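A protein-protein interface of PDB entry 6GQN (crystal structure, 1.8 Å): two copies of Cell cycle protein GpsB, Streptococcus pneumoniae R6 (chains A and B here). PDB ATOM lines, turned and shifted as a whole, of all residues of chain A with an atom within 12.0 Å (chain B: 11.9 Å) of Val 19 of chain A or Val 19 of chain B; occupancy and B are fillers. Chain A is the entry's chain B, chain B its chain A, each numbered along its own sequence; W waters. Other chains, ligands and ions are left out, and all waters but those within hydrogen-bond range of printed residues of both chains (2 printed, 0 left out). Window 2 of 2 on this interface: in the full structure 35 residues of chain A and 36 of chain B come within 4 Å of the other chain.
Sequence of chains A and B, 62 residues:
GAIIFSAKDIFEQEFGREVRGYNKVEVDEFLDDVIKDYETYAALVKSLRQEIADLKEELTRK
Printed residues of chain B that touch a printed residue of chain A: Phe 15, Gly 16, Arg 17, Glu 18, Val 19, Arg 20, Gly 21, Tyr 22, Asn 23, Lys 24, Glu 26 and Val 27. Hydrophobic or aromatic side chains of chain B that line the printed part of chain A: Phe 15, Tyr 22 and Val 27. Among the printed residues, 39 pairs touch across the chains.
Phe 15 of chain A touches Val 27 of chain B, and with the chains exchanged Val 27 of chain A touches Phe 15 of chain B. Gly 16 of chain A touches Glu 26 of chain B, and with the chains exchanged Glu 26 of chain A touches Gly 16 of chain B. Arg 17 of chain A touches Arg 20 of chain B, and with the chains exchanged Arg 20 of chain A touches Arg 17 of chain B. Glu 18 of chain A touches Val 19 of chain B, but with the chains exchanged Val 19 of chain A does not touch Glu 18 of chain B (4.6 Å). Positions printed for both chains: 15, 16, 17, 18, 19, 20, 21, 22, 23, 24, 25, 26 and 27. Of the 39 pairs that touch across the chains among the printed residues, 33 have their exchanged pair printed and touching as well.
The side-chain amide oxygen (OD1) of Asn 23 of chain B is in hydrogen-bond range of the backbone NH (N) of Val 25 of chain B (3.2 Å). OD1 of Asn 23 of chain B is in hydrogen-bond range of N of Glu 26 of chain B. The backbone carbonyl oxygen (O) of Phe 15 of chain A is in hydrogen-bond range of the guanidinium group (NH2) of Arg 17 of chain A (2.8 Å). The side-chain amide oxygen of Asn 23 of chain A lies within hydrogen-bond range of the backbone NH of Val 25 of chain A. The side-chain amide oxygen (OD1) of Asn 23 of chain A sits at hydrogen-bond distance from the backbone NH (N) of Glu 26 of chain A, at 3.0 Å.
Phe 15 of chain A touches Glu 26 of chain B. Arg 17 of chain A touches Tyr 22 of chain B. Glu 18 of chain A touches Tyr 22 of chain B. Gly 21 of chain A touches Arg 17 of chain B. Gly 21 of chain A touches Lys 24 of chain B (CA to CG, 3.9 Å). Tyr 22 of chain A touches Gly 16 of chain B. Lys 24 of chain B touches Tyr 22 of chain A. Tyr 22 of chain A touches Val 27 of chain B. Phe 15 of chain B touches Glu 26 of chain A (CA to OE1, 3.5 Å). CD1 of Phe 15 of chain B touches CG2 of Val 27 of chain A, 3.6 Å away.
The backbone NH (N) of Asn 23 of chain A sits at hydrogen-bond distance from the backbone carbonyl oxygen (O) of Gly 16 of chain B (2.8 Å). The backbone NH of Gly 16 of chain B is in hydrogen-bond range of the side-chain carboxylate of Glu 26 of chain A, 2.9 Å away. N of Arg 20 of chain A sits close to O of Glu 18 of chain B (3.4 Å). The backbone NH (N) of Glu 18 of chain B sits at hydrogen-bond distance from the backbone carbonyl oxygen (O) of Gly 21 of chain A, 3.0 Å away. The backbone NH (N) of Lys 24 of chain A lies within hydrogen-bond range of the side-chain carboxylate (OE2) of Glu 18 of chain B, at 3.0 Å. O of Val 19 of chain B sits at hydrogen-bond distance from N of Arg 20 of chain A (3.0 Å). N of Glu 18 of chain A lies within hydrogen-bond range of O of Gly 21 of chain B (2.8 Å). O of Tyr 22 of chain B lies within hydrogen-bond range of N of Tyr 22 of chain A, at 2.8 Å. NZ of Lys 24 of chain A is in hydrogen-bond range of OH of Tyr 22 of chain B (2.7 Å). The backbone carbonyl oxygen (O) of Gly 16 of chain A lies within hydrogen-bond range of the backbone NH (N) of Asn 23 of chain B (2.8 Å). OE1 of Glu 18 of chain A is in salt-bridge range of NZ of Lys 24 of chain B, at 2.7 Å. The side-chain amino group (NZ) of Lys 24 of chain B is in hydrogen-bond range of the backbone carbonyl oxygen (O) of Arg 20 of chain A. OE1 of Glu 26 of chain B sits at hydrogen-bond distance from N of Gly 16 of chain A, 2.7 Å away.
Water W2 lies within hydrogen-bond range of the backbone carbonyl oxygen of Arg 17 of chain A (2.9 Å) and the side-chain amide nitrogen of Asn 23 of chain B (3.1 Å). Water W1 lies within hydrogen-bond range of the side-chain carboxylate of Glu 18 of chain A (2.9 Å), the backbone NH of Val 25 of chain B (3.1 Å), the backbone NH of Lys 24 of chain B (3.2 Å) and the side-chain amide oxygen of Asn 23 of chain B (3.3 Å).
Of chain B, only Val 19 comes within 4 Å of Val 19 of chain A. Val 19 of chain B touches just these residues of chain A: Glu 18 (3.9 Å), Val 19 (3.1 Å) and Arg 20 (3.0 Å). Of the printed residues of chain A, Arg 17 of chain B touches Arg 20 (3.5 Å) and Gly 21 (3.1 Å). Of chain A, only Arg 20, Gly 21, Asn 23 and Lys 24 come within 4 Å of Glu 18 of chain B. Printed residues of chain A within 4 Å of Tyr 22 of chain B: Phe 15 (3.6 Å), Gly 16 (3.5 Å), Arg 17 (3.6 Å), Glu 18 (3.9 Å), Gly 21 (3.1 Å), Tyr 22 (2.8 Å), Lys 24 (2.7 Å) and Val 27 (3.6 Å). Printed residues of chain B within 4 Å of Glu 26 of chain A: Phe 15 and Gly 16. Printed residues of chain B within 4 Å of Asn 23 of chain A: Gly 16 (2.8 Å) and Glu 18 (3.7 Å). Of the printed residues of chain A, Gly 16 of chain B touches Tyr 22, Asn 23 and Glu 26. The nearest residue of chain A that does not touch Val 19 of chain B is Gly 21 of chain A (4.8 Å).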
ATOM      1  N   PHE A  15      -9.948  11.212 -23.045  1.00  0.00           N
ATOM      2  CA  PHE A  15      -9.979  12.611 -22.672  1.00  0.00           C
ATOM      3  C   PHE A  15      -9.475  13.392 -23.861  1.00  0.00           C
ATOM      4  O   PHE A  15      -8.644  12.884 -24.614  1.00  0.00           O
ATOM      5  CB  PHE A  15      -9.076  12.879 -21.475  1.00  0.00           C
ATOM      6  CG  PHE A  15      -9.449  12.064 -20.255  1.00  0.00           C
ATOM      7  CD1 PHE A  15     -10.576  12.375 -19.523  1.00  0.00           C
ATOM      8  CD2 PHE A  15      -8.675  11.000 -19.856  1.00  0.00           C
ATOM      9  CE1 PHE A  15     -10.922  11.623 -18.371  1.00  0.00           C
ATOM     10  CE2 PHE A  15      -9.013  10.258 -18.674  1.00  0.00           C
ATOM     11  CZ  PHE A  15     -10.161  10.572 -17.974  1.00  0.00           C
ATOM     12  N   GLY A  16      -9.951  14.607 -24.017  1.00  0.00           N
ATOM     13  CA  GLY A  16      -9.309  15.496 -24.981  1.00  0.00           C
ATOM     14  C   GLY A  16      -7.923  15.858 -24.509  1.00  0.00           C
ATOM     15  O   GLY A  16      -7.550  15.671 -23.348  1.00  0.00           O
ATOM     16  N   ARG A  17      -7.159  16.445 -25.416  1.00  0.00           N
ATOM     17  CA  ARG A  17      -5.863  16.990 -25.069  1.00  0.00           C
ATOM     18  C   ARG A  17      -5.978  18.506 -24.993  1.00  0.00           C
ATOM     19  O   ARG A  17      -6.824  19.114 -25.645  1.00  0.00           O
ATOM     20  CB  ARG A  17      -4.794  16.593 -26.092  1.00  0.00           C
ATOM     21  CG  ARG A  17      -4.736  15.113 -26.358  1.00  0.00           C
ATOM     22  CD  ARG A  17      -4.200  14.366 -25.172  1.00  0.00           C
ATOM     23  NE  ARG A  17      -3.899  12.963 -25.475  1.00  0.00           N
ATOM     24  CZ  ARG A  17      -4.770  11.949 -25.406  1.00  0.00           C
ATOM     25  NH1 ARG A  17      -4.383  10.709 -25.682  1.00  0.00           N
ATOM     26  NH2 ARG A  17      -6.027  12.167 -25.087  1.00  0.00           N
ATOM     27  N   GLU A  18      -5.140  19.114 -24.173  1.00  0.00           N
ATOM     28  CA  GLU A  18      -5.033  20.563 -24.196  1.00  0.00           C
ATOM     29  C   GLU A  18      -3.596  20.940 -23.897  1.00  0.00           C
ATOM     30  O   GLU A  18      -2.857  20.176 -23.263  1.00  0.00           O
ATOM     31  CB  GLU A  18      -5.985  21.198 -23.174  1.00  0.00           C
ATOM     32  CG  GLU A  18      -5.657  20.810 -21.791  1.00  0.00           C
ATOM     33  CD  GLU A  18      -6.541  21.518 -20.829  1.00  0.00           C
ATOM     34  OE1 GLU A  18      -6.421  21.281 -19.620  1.00  0.00           O
ATOM     35  OE2 GLU A  18      -7.366  22.316 -21.307  1.00  0.00           O
ATOM     36  N   VAL A  19      -3.190  22.121 -24.350  1.00  0.00           N
ATOM     37  CA  VAL A  19      -1.881  22.596 -23.935  1.00  0.00           C
ATOM     38  C   VAL A  19      -1.951  22.835 -22.446  1.00  0.00           C
ATOM     39  O   VAL A  19      -2.974  23.310 -21.929  1.00  0.00           O
ATOM     40  CB  VAL A  19      -1.450  23.876 -24.671  1.00  0.00           C
ATOM     41  CG1 VAL A  19      -1.057  23.555 -26.107  1.00  0.00           C
ATOM     42  CG2 VAL A  19      -2.528  24.897 -24.634  1.00  0.00           C
ATOM     43  N   ARG A  20      -0.869  22.503 -21.762  1.00  0.00           N
ATOM     44  CA  ARG A  20      -0.770  22.559 -20.314  1.00  0.00           C
ATOM     45  C   ARG A  20      -1.848  21.704 -19.657  1.00  0.00           C
ATOM     46  O   ARG A  20      -2.352  22.042 -18.595  1.00  0.00           O
ATOM     47  CB  ARG A  20      -0.828  23.983 -19.773  1.00  0.00           C
ATOM     48  CG  ARG A  20       0.192  24.929 -20.478  1.00  0.00           C
ATOM     49  CD  ARG A  20       1.614  24.376 -20.324  1.00  0.00           C
ATOM     50  NE  ARG A  20       2.600  25.065 -21.178  1.00  0.00           N
ATOM     51  CZ  ARG A  20       3.890  24.737 -21.197  1.00  0.00           C
ATOM     52  NH1 ARG A  20       4.335  23.762 -20.410  1.00  0.00           N
ATOM     53  NH2 ARG A  20       4.734  25.359 -21.976  1.00  0.00           N
ATOM     54  N   GLY A  21      -2.203  20.589 -20.259  1.00  0.00           N
ATOM     55  CA  GLY A  21      -3.082  19.642 -19.594  1.00  0.00           C
ATOM     56  C   GLY A  21      -2.326  18.775 -18.623  1.00  0.00           C
ATOM     57  O   GLY A  21      -1.136  18.913 -18.405  1.00  0.00           O
ATOM     58  N   TYR A  22      -3.044  17.825 -18.027  1.00  0.00           N
ATOM     59  CA  TYR A  22      -2.413  16.927 -17.085  1.00  0.00           C
ATOM     60  C   TYR A  22      -1.471  15.959 -17.777  1.00  0.00           C
ATOM     61  O   TYR A  22      -1.783  15.411 -18.830  1.00  0.00           O
ATOM     62  CB  TYR A  22      -3.498  16.152 -16.349  1.00  0.00           C
ATOM     63  CG  TYR A  22      -4.269  16.950 -15.339  1.00  0.00           C
ATOM     64  CD1 TYR A  22      -3.642  17.868 -14.524  1.00  0.00           C
ATOM     65  CD2 TYR A  22      -5.635  16.733 -15.159  1.00  0.00           C
ATOM     66  CE1 TYR A  22      -4.332  18.551 -13.555  1.00  0.00           C
ATOM     67  CE2 TYR A  22      -6.330  17.407 -14.176  1.00  0.00           C
ATOM     68  CZ  TYR A  22      -5.676  18.324 -13.401  1.00  0.00           C
ATOM     69  OH  TYR A  22      -6.377  19.023 -12.446  1.00  0.00           O
ATOM     70  N   ASN A  23      -0.329  15.704 -17.144  1.00  0.00           N
ATOM     71  CA  ASN A  23       0.596  14.677 -17.602  1.00  0.00           C
ATOM     72  C   ASN A  23      -0.136  13.347 -17.788  1.00  0.00           C
ATOM     73  O   ASN A  23      -0.740  12.818 -16.849  1.00  0.00           O
ATOM     74  CB  ASN A  23       1.705  14.562 -16.563  1.00  0.00           C
ATOM     75  CG  ASN A  23       2.778  13.594 -16.957  1.00  0.00           C
ATOM     76  OD1 ASN A  23       2.513  12.442 -17.244  1.00  0.00           O
ATOM     77  ND2 ASN A  23       3.996  14.048 -16.916  1.00  0.00           N
ATOM     78  N   LYS A  24      -0.158  12.835 -19.025  1.00  0.00           N
ATOM     79  CA  LYS A  24      -0.972  11.642 -19.326  1.00  0.00           C
ATOM     80  C   LYS A  24      -0.422  10.417 -18.607  1.00  0.00           C
ATOM     81  O   LYS A  24      -1.179   9.520 -18.180  1.00  0.00           O
ATOM     82  CB  LYS A  24      -1.001  11.415 -20.858  1.00  0.00           C
ATOM     83  CG  LYS A  24      -1.500  10.021 -21.298  1.00  0.00           C
ATOM     84  CD  LYS A  24      -1.597   9.889 -22.837  1.00  0.00           C
ATOM     85  CE  LYS A  24      -2.024   8.502 -23.313  1.00  0.00           C
ATOM     86  NZ  LYS A  24      -3.514   8.145 -23.193  1.00  0.00           N
ATOM     87  N   VAL A  25       0.906  10.329 -18.525  1.00  0.00           N
ATOM     88  CA  VAL A  25       1.530   9.182 -17.881  1.00  0.00           C
ATOM     89  C   VAL A  25       1.111   9.128 -16.438  1.00  0.00           C
ATOM     90  O   VAL A  25       0.686   8.068 -15.934  1.00  0.00           O
ATOM     91  CB  VAL A  25       3.061   9.252 -18.037  1.00  0.00           C
ATOM     92  CG1 VAL A  25       3.701   8.120 -17.212  1.00  0.00           C
ATOM     93  CG2 VAL A  25       3.381   9.020 -19.471  1.00  0.00           C
ATOM     94  N   GLU A  26       1.091  10.293 -15.791  1.00  0.00           N
ATOM     95  CA  GLU A  26       0.774  10.369 -14.375  1.00  0.00           C
ATOM     96  C   GLU A  26      -0.689  10.040 -14.154  1.00  0.00           C
ATOM     97  O   GLU A  26      -1.046   9.296 -13.227  1.00  0.00           O
ATOM     98  CB  GLU A  26       1.062  11.772 -13.831  1.00  0.00           C
ATOM     99  CG  GLU A  26       2.500  12.286 -13.893  1.00  0.00           C
ATOM    100  CD  GLU A  26       2.697  13.577 -13.061  1.00  0.00           C
ATOM    101  OE1 GLU A  26       1.804  13.922 -12.263  1.00  0.00           O
ATOM    102  OE2 GLU A  26       3.747  14.258 -13.210  1.00  0.00           O
ATOM    103  N   VAL A  27      -1.564  10.619 -14.967  1.00  0.00           N
ATOM    104  CA  VAL A  27      -2.987  10.278 -14.842  1.00  0.00           C
ATOM    105  C   VAL A  27      -3.215   8.800 -15.089  1.00  0.00           C
ATOM    106  O   VAL A  27      -3.997   8.131 -14.382  1.00  0.00           O
ATOM    107  CB  VAL A  27      -3.822  11.133 -15.815  1.00  0.00           C
ATOM    108  CG1 VAL A  27      -5.238  10.651 -15.777  1.00  0.00           C
ATOM    109  CG2 VAL A  27      -3.777  12.562 -15.367  1.00  0.00           C
ATOM    110  N   PHE B  15      -1.772  16.182 -10.356  1.00  0.00           N
ATOM    111  CA  PHE B  15      -1.034  15.762 -11.530  1.00  0.00           C
ATOM    112  C   PHE B  15      -0.238  16.957 -11.991  1.00  0.00           C
ATOM    113  O   PHE B  15      -0.740  18.082 -11.961  1.00  0.00           O
ATOM    114  CB  PHE B  15      -1.960  15.329 -12.654  1.00  0.00           C
ATOM    115  CG  PHE B  15      -2.980  14.286 -12.229  1.00  0.00           C
ATOM    116  CD1 PHE B  15      -2.582  12.992 -11.955  1.00  0.00           C
ATOM    117  CD2 PHE B  15      -4.308  14.614 -12.112  1.00  0.00           C
ATOM    118  CE1 PHE B  15      -3.509  12.040 -11.545  1.00  0.00           C
ATOM    119  CE2 PHE B  15      -5.238  13.666 -11.728  1.00  0.00           C
ATOM    120  CZ  PHE B  15      -4.825  12.370 -11.444  1.00  0.00           C
ATOM    121  N   GLY B  16       1.001  16.731 -12.363  1.00  0.00           N
ATOM    122  CA  GLY B  16       1.725  17.783 -13.008  1.00  0.00           C
ATOM    123  C   GLY B  16       1.143  18.057 -14.374  1.00  0.00           C
ATOM    124  O   GLY B  16       0.408  17.263 -14.937  1.00  0.00           O
ATOM    125  N   ARG B  17       1.493  19.197 -14.933  1.00  0.00           N
ATOM    126  CA  ARG B  17       1.041  19.524 -16.274  1.00  0.00           C
ATOM    127  C   ARG B  17       2.193  19.262 -17.231  1.00  0.00           C
ATOM    128  O   ARG B  17       3.350  19.383 -16.842  1.00  0.00           O
ATOM    129  CB  ARG B  17       0.602  20.988 -16.376  1.00  0.00           C
ATOM    130  CG  ARG B  17      -0.637  21.340 -15.499  1.00  0.00           C
ATOM    131  CD  ARG B  17      -0.742  22.864 -15.542  1.00  0.00           C
ATOM    132  NE  ARG B  17      -1.899  23.476 -14.879  1.00  0.00           N
ATOM    133  CZ  ARG B  17      -2.244  24.758 -15.056  1.00  0.00           C
ATOM    134  NH1 ARG B  17      -3.303  25.281 -14.436  1.00  0.00           N
ATOM    135  NH2 ARG B  17      -1.531  25.510 -15.885  1.00  0.00           N
ATOM    136  N   GLU B  18       1.867  18.893 -18.467  1.00  0.00           N
ATOM    137  CA  GLU B  18       2.844  18.667 -19.523  1.00  0.00           C
ATOM    138  C   GLU B  18       2.381  19.463 -20.736  1.00  0.00           C
ATOM    139  O   GLU B  18       1.339  20.109 -20.714  1.00  0.00           O
ATOM    140  CB  GLU B  18       3.021  17.165 -19.823  1.00  0.00           C
ATOM    141  CG  GLU B  18       2.059  16.512 -20.855  1.00  0.00           C
ATOM    142  CD  GLU B  18       2.319  14.995 -21.015  1.00  0.00           C
ATOM    143  OE1 GLU B  18       3.493  14.585 -20.903  1.00  0.00           O
ATOM    144  OE2 GLU B  18       1.355  14.206 -21.201  1.00  0.00           O
ATOM    145  N   VAL B  19       3.159  19.450 -21.810  1.00  0.00           N
ATOM    146  CA  VAL B  19       2.923  20.450 -22.832  1.00  0.00           C
ATOM    147  C   VAL B  19       1.596  20.206 -23.554  1.00  0.00           C
ATOM    148  O   VAL B  19       0.878  21.167 -23.874  1.00  0.00           O
ATOM    149  CB  VAL B  19       4.139  20.502 -23.786  1.00  0.00           C
ATOM    150  CG1 VAL B  19       4.126  19.316 -24.722  1.00  0.00           C
ATOM    151  CG2 VAL B  19       4.233  21.856 -24.497  1.00  0.00           C
ATOM    152  N   ARG B  20       1.239  18.941 -23.811  1.00  0.00           N
ATOM    153  CA  ARG B  20       0.049  18.528 -24.575  1.00  0.00           C
ATOM    154  C   ARG B  20      -0.749  17.454 -23.798  1.00  0.00           C
ATOM    155  O   ARG B  20      -1.098  16.387 -24.306  1.00  0.00           O
ATOM    156  CB  ARG B  20       0.428  18.003 -25.958  1.00  0.00           C
ATOM    157  N   GLY B  21      -1.106  17.759 -22.572  1.00  0.00           N
ATOM    158  CA  GLY B  21      -1.671  16.744 -21.681  1.00  0.00           C
ATOM    159  C   GLY B  21      -3.171  16.528 -21.845  1.00  0.00           C
ATOM    160  O   GLY B  21      -3.850  17.071 -22.723  1.00  0.00           O
ATOM    161  N   TYR B  22      -3.688  15.712 -20.937  1.00  0.00           N
ATOM    162  CA  TYR B  22      -5.123  15.551 -20.803  1.00  0.00           C
ATOM    163  C   TYR B  22      -5.803  16.846 -20.435  1.00  0.00           C
ATOM    164  O   TYR B  22      -5.336  17.581 -19.564  1.00  0.00           O
ATOM    165  CB  TYR B  22      -5.431  14.525 -19.700  1.00  0.00           C
ATOM    166  CG  TYR B  22      -5.236  13.100 -20.088  1.00  0.00           C
ATOM    167  CD1 TYR B  22      -5.481  12.656 -21.377  1.00  0.00           C
ATOM    168  CD2 TYR B  22      -4.844  12.175 -19.134  1.00  0.00           C
ATOM    169  CE1 TYR B  22      -5.331  11.352 -21.695  1.00  0.00           C
ATOM    170  CE2 TYR B  22      -4.664  10.865 -19.437  1.00  0.00           C
ATOM    171  CZ  TYR B  22      -4.945  10.448 -20.701  1.00  0.00           C
ATOM    172  OH  TYR B  22      -4.783   9.124 -20.999  1.00  0.00           O
ATOM    173  N   ASN B  23      -6.965  17.078 -21.037  1.00  0.00           N
ATOM    174  CA  ASN B  23      -7.837  18.170 -20.621  1.00  0.00           C
ATOM    175  C   ASN B  23      -8.128  18.070 -19.128  1.00  0.00           C
ATOM    176  O   ASN B  23      -8.696  17.072 -18.672  1.00  0.00           O
ATOM    177  CB  ASN B  23      -9.157  18.092 -21.396  1.00  0.00           C
ATOM    178  CG  ASN B  23     -10.050  19.292 -21.155  1.00  0.00           C
ATOM    179  OD1 ASN B  23     -10.695  19.393 -20.110  1.00  0.00           O
ATOM    180  ND2 ASN B  23     -10.091  20.217 -22.118  1.00  0.00           N
ATOM    181  N   LYS B  24      -7.820  19.131 -18.384  1.00  0.00           N
ATOM    182  CA  LYS B  24      -7.858  19.032 -16.927  1.00  0.00           C
ATOM    183  C   LYS B  24      -9.287  19.018 -16.411  1.00  0.00           C
ATOM    184  O   LYS B  24      -9.600  18.299 -15.457  1.00  0.00           O
ATOM    185  CB  LYS B  24      -7.097  20.191 -16.301  1.00  0.00           C
ATOM    186  CG  LYS B  24      -5.595  20.286 -16.748  1.00  0.00           C
ATOM    187  CD  LYS B  24      -4.839  21.373 -15.977  1.00  0.00           C
ATOM    188  CE  LYS B  24      -5.089  22.787 -16.496  1.00  0.00           C
ATOM    189  NZ  LYS B  24      -4.836  22.784 -17.953  1.00  0.00           N
ATOM    190  N   VAL B  25     -10.161  19.835 -17.009  1.00  0.00           N
ATOM    191  CA  VAL B  25     -11.552  19.891 -16.577  1.00  0.00           C
ATOM    192  C   VAL B  25     -12.231  18.559 -16.816  1.00  0.00           C
ATOM    193  O   VAL B  25     -13.049  18.106 -16.008  1.00  0.00           O
ATOM    194  CB  VAL B  25     -12.297  21.021 -17.306  1.00  0.00           C
ATOM    195  CG1 VAL B  25     -13.805  20.931 -16.985  1.00  0.00           C
ATOM    196  CG2 VAL B  25     -11.742  22.358 -16.852  1.00  0.00           C
ATOM    197  N   GLU B  26     -11.885  17.898 -17.918  1.00  0.00           N
ATOM    198  CA  GLU B  26     -12.464  16.593 -18.214  1.00  0.00           C
ATOM    199  C   GLU B  26     -11.940  15.538 -17.264  1.00  0.00           C
ATOM    200  O   GLU B  26     -12.711  14.719 -16.781  1.00  0.00           O
ATOM    201  CB  GLU B  26     -12.148  16.163 -19.634  1.00  0.00           C
ATOM    202  CG  GLU B  26     -12.879  16.951 -20.715  1.00  0.00           C
ATOM    203  CD  GLU B  26     -12.514  16.454 -22.104  1.00  0.00           C
ATOM    204  OE1 GLU B  26     -11.818  15.417 -22.220  1.00  0.00           O
ATOM    205  OE2 GLU B  26     -12.934  17.100 -23.076  1.00  0.00           O
ATOM    206  N   VAL B  27     -10.634  15.534 -17.000  1.00  0.00           N
ATOM    207  CA  VAL B  27     -10.097  14.590 -16.021  1.00  0.00           C
ATOM    208  C   VAL B  27     -10.767  14.811 -14.667  1.00  0.00           C
ATOM    209  O   VAL B  27     -11.129  13.862 -13.965  1.00  0.00           O
ATOM    210  CB  VAL B  27      -8.568  14.728 -15.933  1.00  0.00           C
ATOM    211  CG1 VAL B  27      -8.021  13.900 -14.749  1.00  0.00           C
ATOM    212  CG2 VAL B  27      -7.905  14.266 -17.278  1.00  0.00           C
HETATM  213  O   HOH W   1      -9.130  22.044 -18.877  1.00  0.00           O
HETATM  214  O   HOH W   2      -9.641  19.254 -25.026  1.00  0.00           O
